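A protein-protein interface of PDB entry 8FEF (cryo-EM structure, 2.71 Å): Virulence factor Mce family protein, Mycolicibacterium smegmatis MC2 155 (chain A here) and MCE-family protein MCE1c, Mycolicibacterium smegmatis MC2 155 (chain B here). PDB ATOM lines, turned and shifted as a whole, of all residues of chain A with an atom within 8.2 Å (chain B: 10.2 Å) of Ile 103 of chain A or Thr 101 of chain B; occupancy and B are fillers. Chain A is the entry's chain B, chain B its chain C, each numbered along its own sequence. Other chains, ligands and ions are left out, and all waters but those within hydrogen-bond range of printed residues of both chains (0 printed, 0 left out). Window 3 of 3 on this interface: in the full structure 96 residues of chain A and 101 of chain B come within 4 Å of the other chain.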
ATOM      1  N   TYR A  99       6.654 -10.346  -8.096  1.00  0.00           N
ATOM      2  CA  TYR A  99       7.366 -10.822  -6.918  1.00  0.00           C
ATOM      3  C   TYR A  99       8.869 -10.723  -7.127  1.00  0.00           C
ATOM      4  O   TYR A  99       9.390 -11.118  -8.172  1.00  0.00           O
ATOM      5  CB  TYR A  99       7.002 -12.277  -6.620  1.00  0.00           C
ATOM      6  CG  TYR A  99       5.712 -12.508  -5.870  1.00  0.00           C
ATOM      7  CD1 TYR A  99       4.686 -11.577  -5.891  1.00  0.00           C
ATOM      8  CD2 TYR A  99       5.525 -13.670  -5.133  1.00  0.00           C
ATOM      9  CE1 TYR A  99       3.510 -11.800  -5.202  1.00  0.00           C
ATOM     10  CE2 TYR A  99       4.358 -13.898  -4.443  1.00  0.00           C
ATOM     11  CZ  TYR A  99       3.354 -12.962  -4.479  1.00  0.00           C
ATOM     12  OH  TYR A  99       2.188 -13.190  -3.789  1.00  0.00           O
ATOM     13  N   GLN A 100       9.568 -10.199  -6.126  1.00  0.00           N
ATOM     14  CA  GLN A 100      11.017 -10.327  -6.093  1.00  0.00           C
ATOM     15  C   GLN A 100      11.446 -11.627  -5.430  1.00  0.00           C
ATOM     16  O   GLN A 100      12.437 -12.235  -5.850  1.00  0.00           O
ATOM     17  CB  GLN A 100      11.645  -9.134  -5.367  1.00  0.00           C
ATOM     18  CG  GLN A 100      13.156  -9.203  -5.242  1.00  0.00           C
ATOM     19  CD  GLN A 100      13.718  -8.138  -4.324  1.00  0.00           C
ATOM     20  OE1 GLN A 100      13.120  -7.079  -4.145  1.00  0.00           O
ATOM     21  NE2 GLN A 100      14.871  -8.418  -3.731  1.00  0.00           N
ATOM     22  N   ASP A 101      10.698 -12.076  -4.429  1.00  0.00           N
ATOM     23  CA  ASP A 101      10.978 -13.318  -3.724  1.00  0.00           C
ATOM     24  C   ASP A 101       9.688 -13.795  -3.066  1.00  0.00           C
ATOM     25  O   ASP A 101       8.610 -13.237  -3.299  1.00  0.00           O
ATOM     26  CB  ASP A 101      12.108 -13.123  -2.710  1.00  0.00           C
ATOM     27  CG  ASP A 101      11.902 -11.905  -1.828  1.00  0.00           C
ATOM     28  OD1 ASP A 101      10.757 -11.425  -1.714  1.00  0.00           O
ATOM     29  OD2 ASP A 101      12.892 -11.415  -1.248  1.00  0.00           O
ATOM     30  N   LEU A 102       9.798 -14.826  -2.235  1.00  0.00           N
ATOM     31  CA  LEU A 102       8.651 -15.399  -1.546  1.00  0.00           C
ATOM     32  C   LEU A 102       8.475 -14.863  -0.130  1.00  0.00           C
ATOM     33  O   LEU A 102       7.649 -15.393   0.618  1.00  0.00           O
ATOM     34  CB  LEU A 102       8.763 -16.924  -1.518  1.00  0.00           C
ATOM     35  CG  LEU A 102       8.685 -17.635  -2.870  1.00  0.00           C
ATOM     36  CD1 LEU A 102       8.872 -19.132  -2.703  1.00  0.00           C
ATOM     37  CD2 LEU A 102       7.365 -17.335  -3.558  1.00  0.00           C
ATOM     38  N   ILE A 103       9.228 -13.834   0.259  1.00  0.00           N
ATOM     39  CA  ILE A 103       9.117 -13.265   1.597  1.00  0.00           C
ATOM     40  C   ILE A 103       8.490 -11.875   1.580  1.00  0.00           C
ATOM     41  O   ILE A 103       8.440 -11.212   2.621  1.00  0.00           O
ATOM     42  CB  ILE A 103      10.475 -13.244   2.318  1.00  0.00           C
ATOM     43  CG1 ILE A 103      11.489 -12.411   1.537  1.00  0.00           C
ATOM     44  CG2 ILE A 103      10.989 -14.659   2.521  1.00  0.00           C
ATOM     45  CD1 ILE A 103      12.852 -12.347   2.184  1.00  0.00           C
ATOM     46  N   GLY A 104       8.007 -11.414   0.429  1.00  0.00           N
ATOM     47  CA  GLY A 104       7.222 -10.196   0.391  1.00  0.00           C
ATOM     48  C   GLY A 104       7.800  -9.012  -0.360  1.00  0.00           C
ATOM     49  O   GLY A 104       7.232  -7.918  -0.306  1.00  0.00           O
ATOM     50  N   ASN A 105       8.914  -9.198  -1.060  1.00  0.00           N
ATOM     51  CA  ASN A 105       9.519  -8.114  -1.821  1.00  0.00           C
ATOM     52  C   ASN A 105       8.934  -8.069  -3.226  1.00  0.00           C
ATOM     53  O   ASN A 105       8.670  -9.109  -3.836  1.00  0.00           O
ATOM     54  CB  ASN A 105      11.038  -8.272  -1.886  1.00  0.00           C
ATOM     55  CG  ASN A 105      11.683  -8.266  -0.517  1.00  0.00           C
ATOM     56  OD1 ASN A 105      11.176  -7.647   0.417  1.00  0.00           O
ATOM     57  ND2 ASN A 105      12.807  -8.957  -0.389  1.00  0.00           N
ATOM     58  N   ARG A 106       8.738  -6.857  -3.738  1.00  0.00           N
ATOM     59  CA  ARG A 106       8.085  -6.629  -5.018  1.00  0.00           C
ATOM     60  C   ARG A 106       8.952  -5.728  -5.884  1.00  0.00           C
ATOM     61  O   ARG A 106       9.931  -5.138  -5.423  1.00  0.00           O
ATOM     62  CB  ARG A 106       6.701  -5.993  -4.838  1.00  0.00           C
ATOM     63  CG  ARG A 106       5.787  -6.714  -3.869  1.00  0.00           C
ATOM     64  CD  ARG A 106       5.147  -7.929  -4.504  1.00  0.00           C
ATOM     65  NE  ARG A 106       4.271  -8.620  -3.568  1.00  0.00           N
ATOM     66  CZ  ARG A 106       4.632  -9.663  -2.835  1.00  0.00           C
ATOM     67  NH1 ARG A 106       5.846 -10.180  -2.921  1.00  0.00           N
ATOM     68  NH2 ARG A 106       3.753 -10.202  -1.996  1.00  0.00           N
ATOM     69  N   LEU A 136      -1.540 -14.223  -3.069  1.00  0.00           N
ATOM     70  CA  LEU A 136      -1.514 -15.612  -2.616  1.00  0.00           C
ATOM     71  C   LEU A 136      -2.746 -15.999  -1.804  1.00  0.00           C
ATOM     72  O   LEU A 136      -3.184 -17.153  -1.859  1.00  0.00           O
ATOM     73  CB  LEU A 136      -0.250 -15.853  -1.789  1.00  0.00           C
ATOM     74  CG  LEU A 136      -0.036 -17.246  -1.197  1.00  0.00           C
ATOM     75  CD1 LEU A 136       0.411 -18.223  -2.269  1.00  0.00           C
ATOM     76  CD2 LEU A 136       0.962 -17.191  -0.060  1.00  0.00           C
ATOM     77  N   ASP A 137      -3.308 -15.060  -1.038  1.00  0.00           N
ATOM     78  CA  ASP A 137      -4.486 -15.379  -0.237  1.00  0.00           C
ATOM     79  C   ASP A 137      -5.666 -15.765  -1.117  1.00  0.00           C
ATOM     80  O   ASP A 137      -6.413 -16.694  -0.792  1.00  0.00           O
ATOM     81  CB  ASP A 137      -4.860 -14.202   0.657  1.00  0.00           C
ATOM     82  CG  ASP A 137      -6.128 -14.458   1.446  1.00  0.00           C
ATOM     83  OD1 ASP A 137      -6.107 -15.324   2.345  1.00  0.00           O
ATOM     84  OD2 ASP A 137      -7.148 -13.794   1.170  1.00  0.00           O
ATOM     85  N   VAL A 140      -5.080 -19.316  -2.375  1.00  0.00           N
ATOM     86  CA  VAL A 140      -5.357 -20.341  -1.374  1.00  0.00           C
ATOM     87  C   VAL A 140      -6.857 -20.457  -1.129  1.00  0.00           C
ATOM     88  O   VAL A 140      -7.392 -21.563  -0.996  1.00  0.00           O
ATOM     89  CB  VAL A 140      -4.582 -20.047  -0.077  1.00  0.00           C
ATOM     90  CG1 VAL A 140      -4.906 -21.081   0.983  1.00  0.00           C
ATOM     91  CG2 VAL A 140      -3.091 -20.033  -0.349  1.00  0.00           C
ATOM     92  N   GLY B  50      -6.860 -15.533  12.805  1.00  0.00           N
ATOM     93  CA  GLY B  50      -6.210 -16.194  11.685  1.00  0.00           C
ATOM     94  C   GLY B  50      -4.703 -16.060  11.674  1.00  0.00           C
ATOM     95  O   GLY B  50      -4.109 -15.849  10.610  1.00  0.00           O
ATOM     96  N   ASP B  56       1.212  -6.274  12.654  1.00  0.00           N
ATOM     97  CA  ASP B  56       1.051  -6.683  11.269  1.00  0.00           C
ATOM     98  C   ASP B  56       0.513  -5.527  10.431  1.00  0.00           C
ATOM     99  O   ASP B  56      -0.136  -4.607  10.934  1.00  0.00           O
ATOM    100  CB  ASP B  56       0.120  -7.889  11.166  1.00  0.00           C
ATOM    101  CG  ASP B  56       0.801  -9.183  11.560  1.00  0.00           C
ATOM    102  OD1 ASP B  56       2.030  -9.292  11.369  1.00  0.00           O
ATOM    103  OD2 ASP B  56       0.108 -10.094  12.057  1.00  0.00           O
ATOM    104  N   LYS B  57       0.794  -5.586   9.133  1.00  0.00           N
ATOM    105  CA  LYS B  57       0.455  -4.489   8.241  1.00  0.00           C
ATOM    106  C   LYS B  57      -1.045  -4.424   7.978  1.00  0.00           C
ATOM    107  O   LYS B  57      -1.728  -5.449   7.894  1.00  0.00           O
ATOM    108  CB  LYS B  57       1.211  -4.631   6.920  1.00  0.00           C
ATOM    109  CG  LYS B  57       2.729  -4.706   7.054  1.00  0.00           C
ATOM    110  CD  LYS B  57       3.348  -3.360   7.410  1.00  0.00           C
ATOM    111  CE  LYS B  57       3.782  -3.302   8.870  1.00  0.00           C
ATOM    112  NZ  LYS B  57       4.363  -1.979   9.229  1.00  0.00           N
ATOM    113  N   ARG B  59      -3.478  -2.692   5.074  1.00  0.00           N
ATOM    114  CA  ARG B  59      -3.319  -2.086   3.763  1.00  0.00           C
ATOM    115  C   ARG B  59      -4.602  -1.646   3.117  1.00  0.00           C
ATOM    116  O   ARG B  59      -5.674  -2.133   3.437  1.00  0.00           O
ATOM    117  CB  ARG B  59      -2.678  -3.076   2.808  1.00  0.00           C
ATOM    118  CG  ARG B  59      -1.342  -3.616   3.237  1.00  0.00           C
ATOM    119  CD  ARG B  59      -0.760  -4.423   2.101  1.00  0.00           C
ATOM    120  NE  ARG B  59       0.598  -4.850   2.372  1.00  0.00           N
ATOM    121  CZ  ARG B  59       1.188  -5.850   1.738  1.00  0.00           C
ATOM    122  NH1 ARG B  59       0.528  -6.517   0.807  1.00  0.00           N
ATOM    123  NH2 ARG B  59       2.429  -6.185   2.037  1.00  0.00           N
ATOM    124  N   ARG B  98      -5.712 -11.679   5.584  1.00  0.00           N
ATOM    125  CA  ARG B  98      -5.250 -12.455   4.449  1.00  0.00           C
ATOM    126  C   ARG B  98      -3.817 -12.910   4.668  1.00  0.00           C
ATOM    127  O   ARG B  98      -3.020 -12.234   5.327  1.00  0.00           O
ATOM    128  CB  ARG B  98      -5.355 -11.652   3.149  1.00  0.00           C
ATOM    129  CG  ARG B  98      -4.639 -10.325   3.165  1.00  0.00           C
ATOM    130  CD  ARG B  98      -4.651  -9.701   1.786  1.00  0.00           C
ATOM    131  NE  ARG B  98      -3.947 -10.520   0.810  1.00  0.00           N
ATOM    132  CZ  ARG B  98      -2.637 -10.480   0.608  1.00  0.00           C
ATOM    133  NH1 ARG B  98      -1.856  -9.671   1.304  1.00  0.00           N
ATOM    134  NH2 ARG B  98      -2.098 -11.270  -0.315  1.00  0.00           N
ATOM    135  N   THR B  99      -3.503 -14.070   4.098  1.00  0.00           N
ATOM    136  CA  THR B  99      -2.158 -14.627   4.145  1.00  0.00           C
ATOM    137  C   THR B  99      -1.280 -13.893   3.141  1.00  0.00           C
ATOM    138  O   THR B  99      -1.601 -13.843   1.949  1.00  0.00           O
ATOM    139  CB  THR B  99      -2.192 -16.122   3.837  1.00  0.00           C
ATOM    140  OG1 THR B  99      -3.090 -16.780   4.740  1.00  0.00           O
ATOM    141  CG2 THR B  99      -0.811 -16.729   3.982  1.00  0.00           C
ATOM    142  N   ASP B 100      -0.174 -13.328   3.616  1.00  0.00           N
ATOM    143  CA  ASP B 100       0.697 -12.541   2.753  1.00  0.00           C
ATOM    144  C   ASP B 100       1.727 -13.403   2.032  1.00  0.00           C
ATOM    145  O   ASP B 100       1.891 -13.288   0.815  1.00  0.00           O
ATOM    146  CB  ASP B 100       1.397 -11.454   3.573  1.00  0.00           C
ATOM    147  CG  ASP B 100       2.106 -10.435   2.706  1.00  0.00           C
ATOM    148  OD1 ASP B 100       1.784 -10.350   1.502  1.00  0.00           O
ATOM    149  OD2 ASP B 100       2.991  -9.725   3.227  1.00  0.00           O
ATOM    150  N   THR B 101       2.425 -14.267   2.765  1.00  0.00           N
ATOM    151  CA  THR B 101       3.492 -15.090   2.215  1.00  0.00           C
ATOM    152  C   THR B 101       3.253 -16.548   2.582  1.00  0.00           C
ATOM    153  O   THR B 101       2.393 -16.876   3.403  1.00  0.00           O
ATOM    154  CB  THR B 101       4.870 -14.637   2.718  1.00  0.00           C
ATOM    155  OG1 THR B 101       4.898 -14.681   4.149  1.00  0.00           O
ATOM    156  CG2 THR B 101       5.175 -13.222   2.255  1.00  0.00           C
ATOM    157  N   ILE B 102       4.032 -17.435   1.956  1.00  0.00           N
ATOM    158  CA  ILE B 102       3.890 -18.863   2.212  1.00  0.00           C
ATOM    159  C   ILE B 102       4.426 -19.255   3.581  1.00  0.00           C
ATOM    160  O   ILE B 102       4.086 -20.329   4.089  1.00  0.00           O
ATOM    161  CB  ILE B 102       4.594 -19.686   1.118  1.00  0.00           C
ATOM    162  CG1 ILE B 102       6.099 -19.426   1.147  1.00  0.00           C
ATOM    163  CG2 ILE B 102       4.019 -19.362  -0.249  1.00  0.00           C
ATOM    164  CD1 ILE B 102       6.885 -20.308   0.217  1.00  0.00           C
ATOM    165  N   LEU B 103       5.258 -18.417   4.195  1.00  0.00           N
ATOM    166  CA  LEU B 103       5.829 -18.730   5.499  1.00  0.00           C
ATOM    167  C   LEU B 103       4.916 -18.351   6.656  1.00  0.00           C
ATOM    168  O   LEU B 103       5.280 -18.595   7.811  1.00  0.00           O
ATOM    169  CB  LEU B 103       7.187 -18.045   5.658  1.00  0.00           C
ATOM    170  CG  LEU B 103       8.311 -18.611   4.788  1.00  0.00           C
ATOM    171  CD1 LEU B 103       9.625 -17.909   5.076  1.00  0.00           C
ATOM    172  CD2 LEU B 103       8.446 -20.108   4.998  1.00  0.00           C
ATOM    173  N   GLY B 104       3.754 -17.766   6.384  1.00  0.00           N
ATOM    174  CA  GLY B 104       2.749 -17.545   7.401  1.00  0.00           C
ATOM    175  C   GLY B 104       2.471 -16.106   7.780  1.00  0.00           C
ATOM    176  O   GLY B 104       1.747 -15.878   8.756  1.00  0.00           O
ATOM    177  N   ARG B 105       3.019 -15.133   7.059  1.00  0.00           N
ATOM    178  CA  ARG B 105       2.753 -13.737   7.381  1.00  0.00           C
ATOM    179  C   ARG B 105       1.321 -13.366   7.019  1.00  0.00           C
ATOM    180  O   ARG B 105       0.807 -13.756   5.967  1.00  0.00           O
ATOM    181  CB  ARG B 105       3.735 -12.823   6.651  1.00  0.00           C
ATOM    182  CG  ARG B 105       5.194 -13.064   7.008  1.00  0.00           C
ATOM    183  CD  ARG B 105       5.413 -13.083   8.514  1.00  0.00           C
ATOM    184  NE  ARG B 105       4.931 -11.871   9.163  1.00  0.00           N
ATOM    185  CZ  ARG B 105       5.651 -10.770   9.322  1.00  0.00           C
ATOM    186  NH1 ARG B 105       6.893 -10.686   8.877  1.00  0.00           N
ATOM    187  NH2 ARG B 105       5.111  -9.725   9.945  1.00  0.00           N
ATOM    188  N   LYS B 106       0.677 -12.606   7.899  1.00  0.00           N
ATOM    189  CA  LYS B 106      -0.705 -12.189   7.727  1.00  0.00           C
ATOM    190  C   LYS B 106      -0.786 -10.670   7.702  1.00  0.00           C
ATOM    191  O   LYS B 106       0.056  -9.979   8.283  1.00  0.00           O
ATOM    192  CB  LYS B 106      -1.596 -12.735   8.849  1.00  0.00           C
ATOM    193  CG  LYS B 106      -1.481 -14.231   9.070  1.00  0.00           C
ATOM    194  CD  LYS B 106      -2.063 -15.013   7.908  1.00  0.00           C
ATOM    195  CE  LYS B 106      -1.805 -16.499   8.067  1.00  0.00           C
ATOM    196  NZ  LYS B 106      -2.330 -17.017   9.358  1.00  0.00           N
ATOM    197  N   ASN B 107      -1.807 -10.151   7.024  1.00  0.00           N
ATOM    198  CA  ASN B 107      -2.034  -8.713   7.011  1.00  0.00           C
ATOM    199  C   ASN B 107      -3.505  -8.434   6.747  1.00  0.00           C
ATOM    200  O   ASN B 107      -4.239  -9.288   6.246  1.00  0.00           O
ATOM    201  CB  ASN B 107      -1.151  -8.006   5.973  1.00  0.00           C
ATOM    202  CG  ASN B 107      -1.542  -8.332   4.547  1.00  0.00           C
ATOM    203  OD1 ASN B 107      -1.066  -9.306   3.971  1.00  0.00           O
ATOM    204  ND2 ASN B 107      -2.397  -7.504   3.964  1.00  0.00           N
ATOM    205  N   PRO B 132      -9.166 -15.581   6.731  1.00  0.00           N
ATOM    206  CA  PRO B 132      -8.479 -16.301   5.658  1.00  0.00           C
ATOM    207  C   PRO B 132      -8.771 -17.792   5.688  1.00  0.00           C
ATOM    208  O   PRO B 132      -9.144 -18.369   6.711  1.00  0.00           O
ATOM    209  CB  PRO B 132      -7.000 -16.025   5.940  1.00  0.00           C
ATOM    210  CG  PRO B 132      -6.944 -15.837   7.405  1.00  0.00           C
ATOM    211  CD  PRO B 132      -8.228 -15.146   7.782  1.00  0.00           C
ATOM    212  N   TYR B 133      -8.598 -18.415   4.526  1.00  0.00           N
ATOM    213  CA  TYR B 133      -8.595 -19.868   4.410  1.00  0.00           C
ATOM    214  C   TYR B 133      -7.156 -20.335   4.591  1.00  0.00           C
ATOM    215  O   TYR B 133      -6.307 -20.102   3.725  1.00  0.00           O
ATOM    216  CB  TYR B 133      -9.164 -20.307   3.064  1.00  0.00           C
ATOM    217  CG  TYR B 133      -9.248 -21.806   2.882  1.00  0.00           C
ATOM    218  CD1 TYR B 133     -10.033 -22.585   3.721  1.00  0.00           C
ATOM    219  CD2 TYR B 133      -8.555 -22.439   1.861  1.00  0.00           C
ATOM    220  CE1 TYR B 133     -10.115 -23.953   3.553  1.00  0.00           C
ATOM    221  CE2 TYR B 133      -8.633 -23.803   1.685  1.00  0.00           C
ATOM    222  CZ  TYR B 133      -9.414 -24.556   2.533  1.00  0.00           C
ATOM    223  OH  TYR B 133      -9.493 -25.917   2.358  1.00  0.00           O
ATOM    224  N   GLN B 134      -6.879 -20.969   5.725  1.00  0.00           N
ATOM    225  CA  GLN B 134      -5.510 -21.277   6.107  1.00  0.00           C
ATOM    226  C   GLN B 134      -4.892 -22.311   5.174  1.00  0.00           C
ATOM    227  O   GLN B 134      -5.580 -23.168   4.615  1.00  0.00           O
ATOM    228  CB  GLN B 134      -5.465 -21.783   7.545  1.00  0.00           C
ATOM    229  CG  GLN B 134      -6.182 -20.893   8.545  1.00  0.00           C
ATOM    230  CD  GLN B 134      -5.466 -19.582   8.795  1.00  0.00           C
ATOM    231  OE1 GLN B 134      -4.313 -19.402   8.410  1.00  0.00           O
ATOM    232  NE2 GLN B 134      -6.154 -18.656   9.448  1.00  0.00           N
ATOM    233  N   ILE B 135      -3.572 -22.216   5.006  1.00  0.00           N
ATOM    234  CA  ILE B 135      -2.856 -23.181   4.179  1.00  0.00           C
ATOM    235  C   ILE B 135      -2.883 -24.562   4.826  1.00  0.00           C
ATOM    236  O   ILE B 135      -3.010 -25.583   4.137  1.00  0.00           O
ATOM    237  CB  ILE B 135      -1.419 -22.695   3.921  1.00  0.00           C
ATOM    238  CG1 ILE B 135      -1.438 -21.341   3.208  1.00  0.00           C
ATOM    239  CG2 ILE B 135      -0.654 -23.701   3.091  1.00  0.00           C
ATOM    240  CD1 ILE B 135      -0.072 -20.856   2.773  1.00  0.00           C
ATOM    241  N   TYR B 136      -2.776 -24.619   6.157  1.00  0.00           N
ATOM    242  CA  TYR B 136      -2.878 -25.906   6.833  1.00  0.00           C
ATOM    243  C   TYR B 136      -4.278 -26.490   6.709  1.00  0.00           C
ATOM    244  O   TYR B 136      -4.427 -27.712   6.609  1.00  0.00           O
ATOM    245  CB  TYR B 136      -2.450 -25.791   8.299  1.00  0.00           C
ATOM    246  CG  TYR B 136      -3.257 -24.858   9.180  1.00  0.00           C
ATOM    247  CD1 TYR B 136      -4.444 -25.273   9.769  1.00  0.00           C
ATOM    248  CD2 TYR B 136      -2.803 -23.578   9.460  1.00  0.00           C
ATOM    249  CE1 TYR B 136      -5.171 -24.430  10.583  1.00  0.00           C
ATOM    250  CE2 TYR B 136      -3.521 -22.730  10.278  1.00  0.00           C
ATOM    251  CZ  TYR B 136      -4.705 -23.161  10.834  1.00  0.00           C
ATOM    252  OH  TYR B 136      -5.427 -22.319  11.647  1.00  0.00           O
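OD1 of Asp 137 of chain A is in hydrogen-bond range of N of Thr 99 of chain B (3.4 Å).
OG1 of Thr 101 of chain B lies close to N of Arg 105 of chain B. The side-chain carboxylate of Asp 101 of chain A sits close to the backbone NH of Ile 103 of chain A. OD1 of Asp 100 of chain B is in salt-bridge range of NH1 of Arg 98 of chain B (3.7 Å). The guanidinium group of Arg 98 of chain B lies within hydrogen-bond range of the side-chain amide oxygen of Asn 107 of chain B (2.8 Å). OD1 of Asp 101 of chain A lies within hydrogen-bond range of N of Gly 104 of chain A (3.5 Å).
Leu 102 of chain A touches Thr 101 of chain B. CD1 of Ile 102 of chain B touches CD1 of Leu 102 of chain A (3.7 Å). Ile 103 of chain A touches Thr 101 of chain B. Thr 101 of chain B touches Gly 104 of chain A (CG2 to N, 3.8 Å). CD2 of Leu 136 of chain A touches C of Thr 101 of chain B (3.6 Å). CD2 of Leu 136 of chain A touches N of Ile 102 of chain B, at 3.7 Å. CG of Asp 137 of chain A touches CB of Arg 98 of chain B, at 3.4 Å. Asp 137 of chain A touches Pro 132 of chain B. O of Val 140 of chain A touches CD2 of Tyr 133 of chain B (3.2 Å).
Of chain B, only Thr 101 (3.6 Å) and Ile 102 (3.7 Å) come within 4 Å of Leu 102 of chain A. Ile 103 of chain A touches one residue of chain B. Of chain B, only Thr 101 comes within 4 Å of Gly 104 of chain A. No residue of chain B comes within 4 Å of Asn 105 of chain A. Of the printed residues of chain B, Val 140 of chain A touches Tyr 133 (3.2 Å). Asp 56 of chain B touches none of the printed residues of chain A. Printed residues of chain A within 4 Å of Arg 98 of chain B: Asp 137. Thr 101 of chain B touches just these residues of chain A: Leu 102, Ile 103, Gly 104 and Leu 136. Of the printed residues of chain A, Ile 102 of chain B touches Leu 102 (3.7 Å) and Leu 136 (3.7 Å). Leu 103 of chain B touches none of the printed residues of chain A. The nearest residue of chain B that does not touch Ile 103 of chain A is Leu 103 of chain B (4.4 Å). The nearest residue of chain A that does not touch Thr 101 of chain B is Arg 106 of chain A (5.4 Å). The nearest printed residue of chain A that does not touch Ile 102 of chain B is Ile 103 of chain A (6.5 Å).
Printed residues of chain B that touch a printed residue of chain A: Arg 98, Thr 99, Thr 101, Ile 102, Pro 132 and Tyr 133. Hydrophobic or aromatic side chains of chain B within 4 Å of the printed part of chain A: Ile 102, Pro 132 and Tyr 133. Of the 11 printed residues of chain A, 6 touch a printed residue of chain B. Printed residues of chain A that touch a printed residue of chain B: Leu 102, Ile 103, Gly 104, Leu 136, Asp 137 and Val 140. Hydrophobic or aromatic side chains of chain A that line the printed part of chain B: Leu 102, Leu 136 and Val 140. Among the printed residues, no Asp or Glu carboxylate lies within 4 Å of a Lys or Arg side-chain nitrogen of the other chain.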
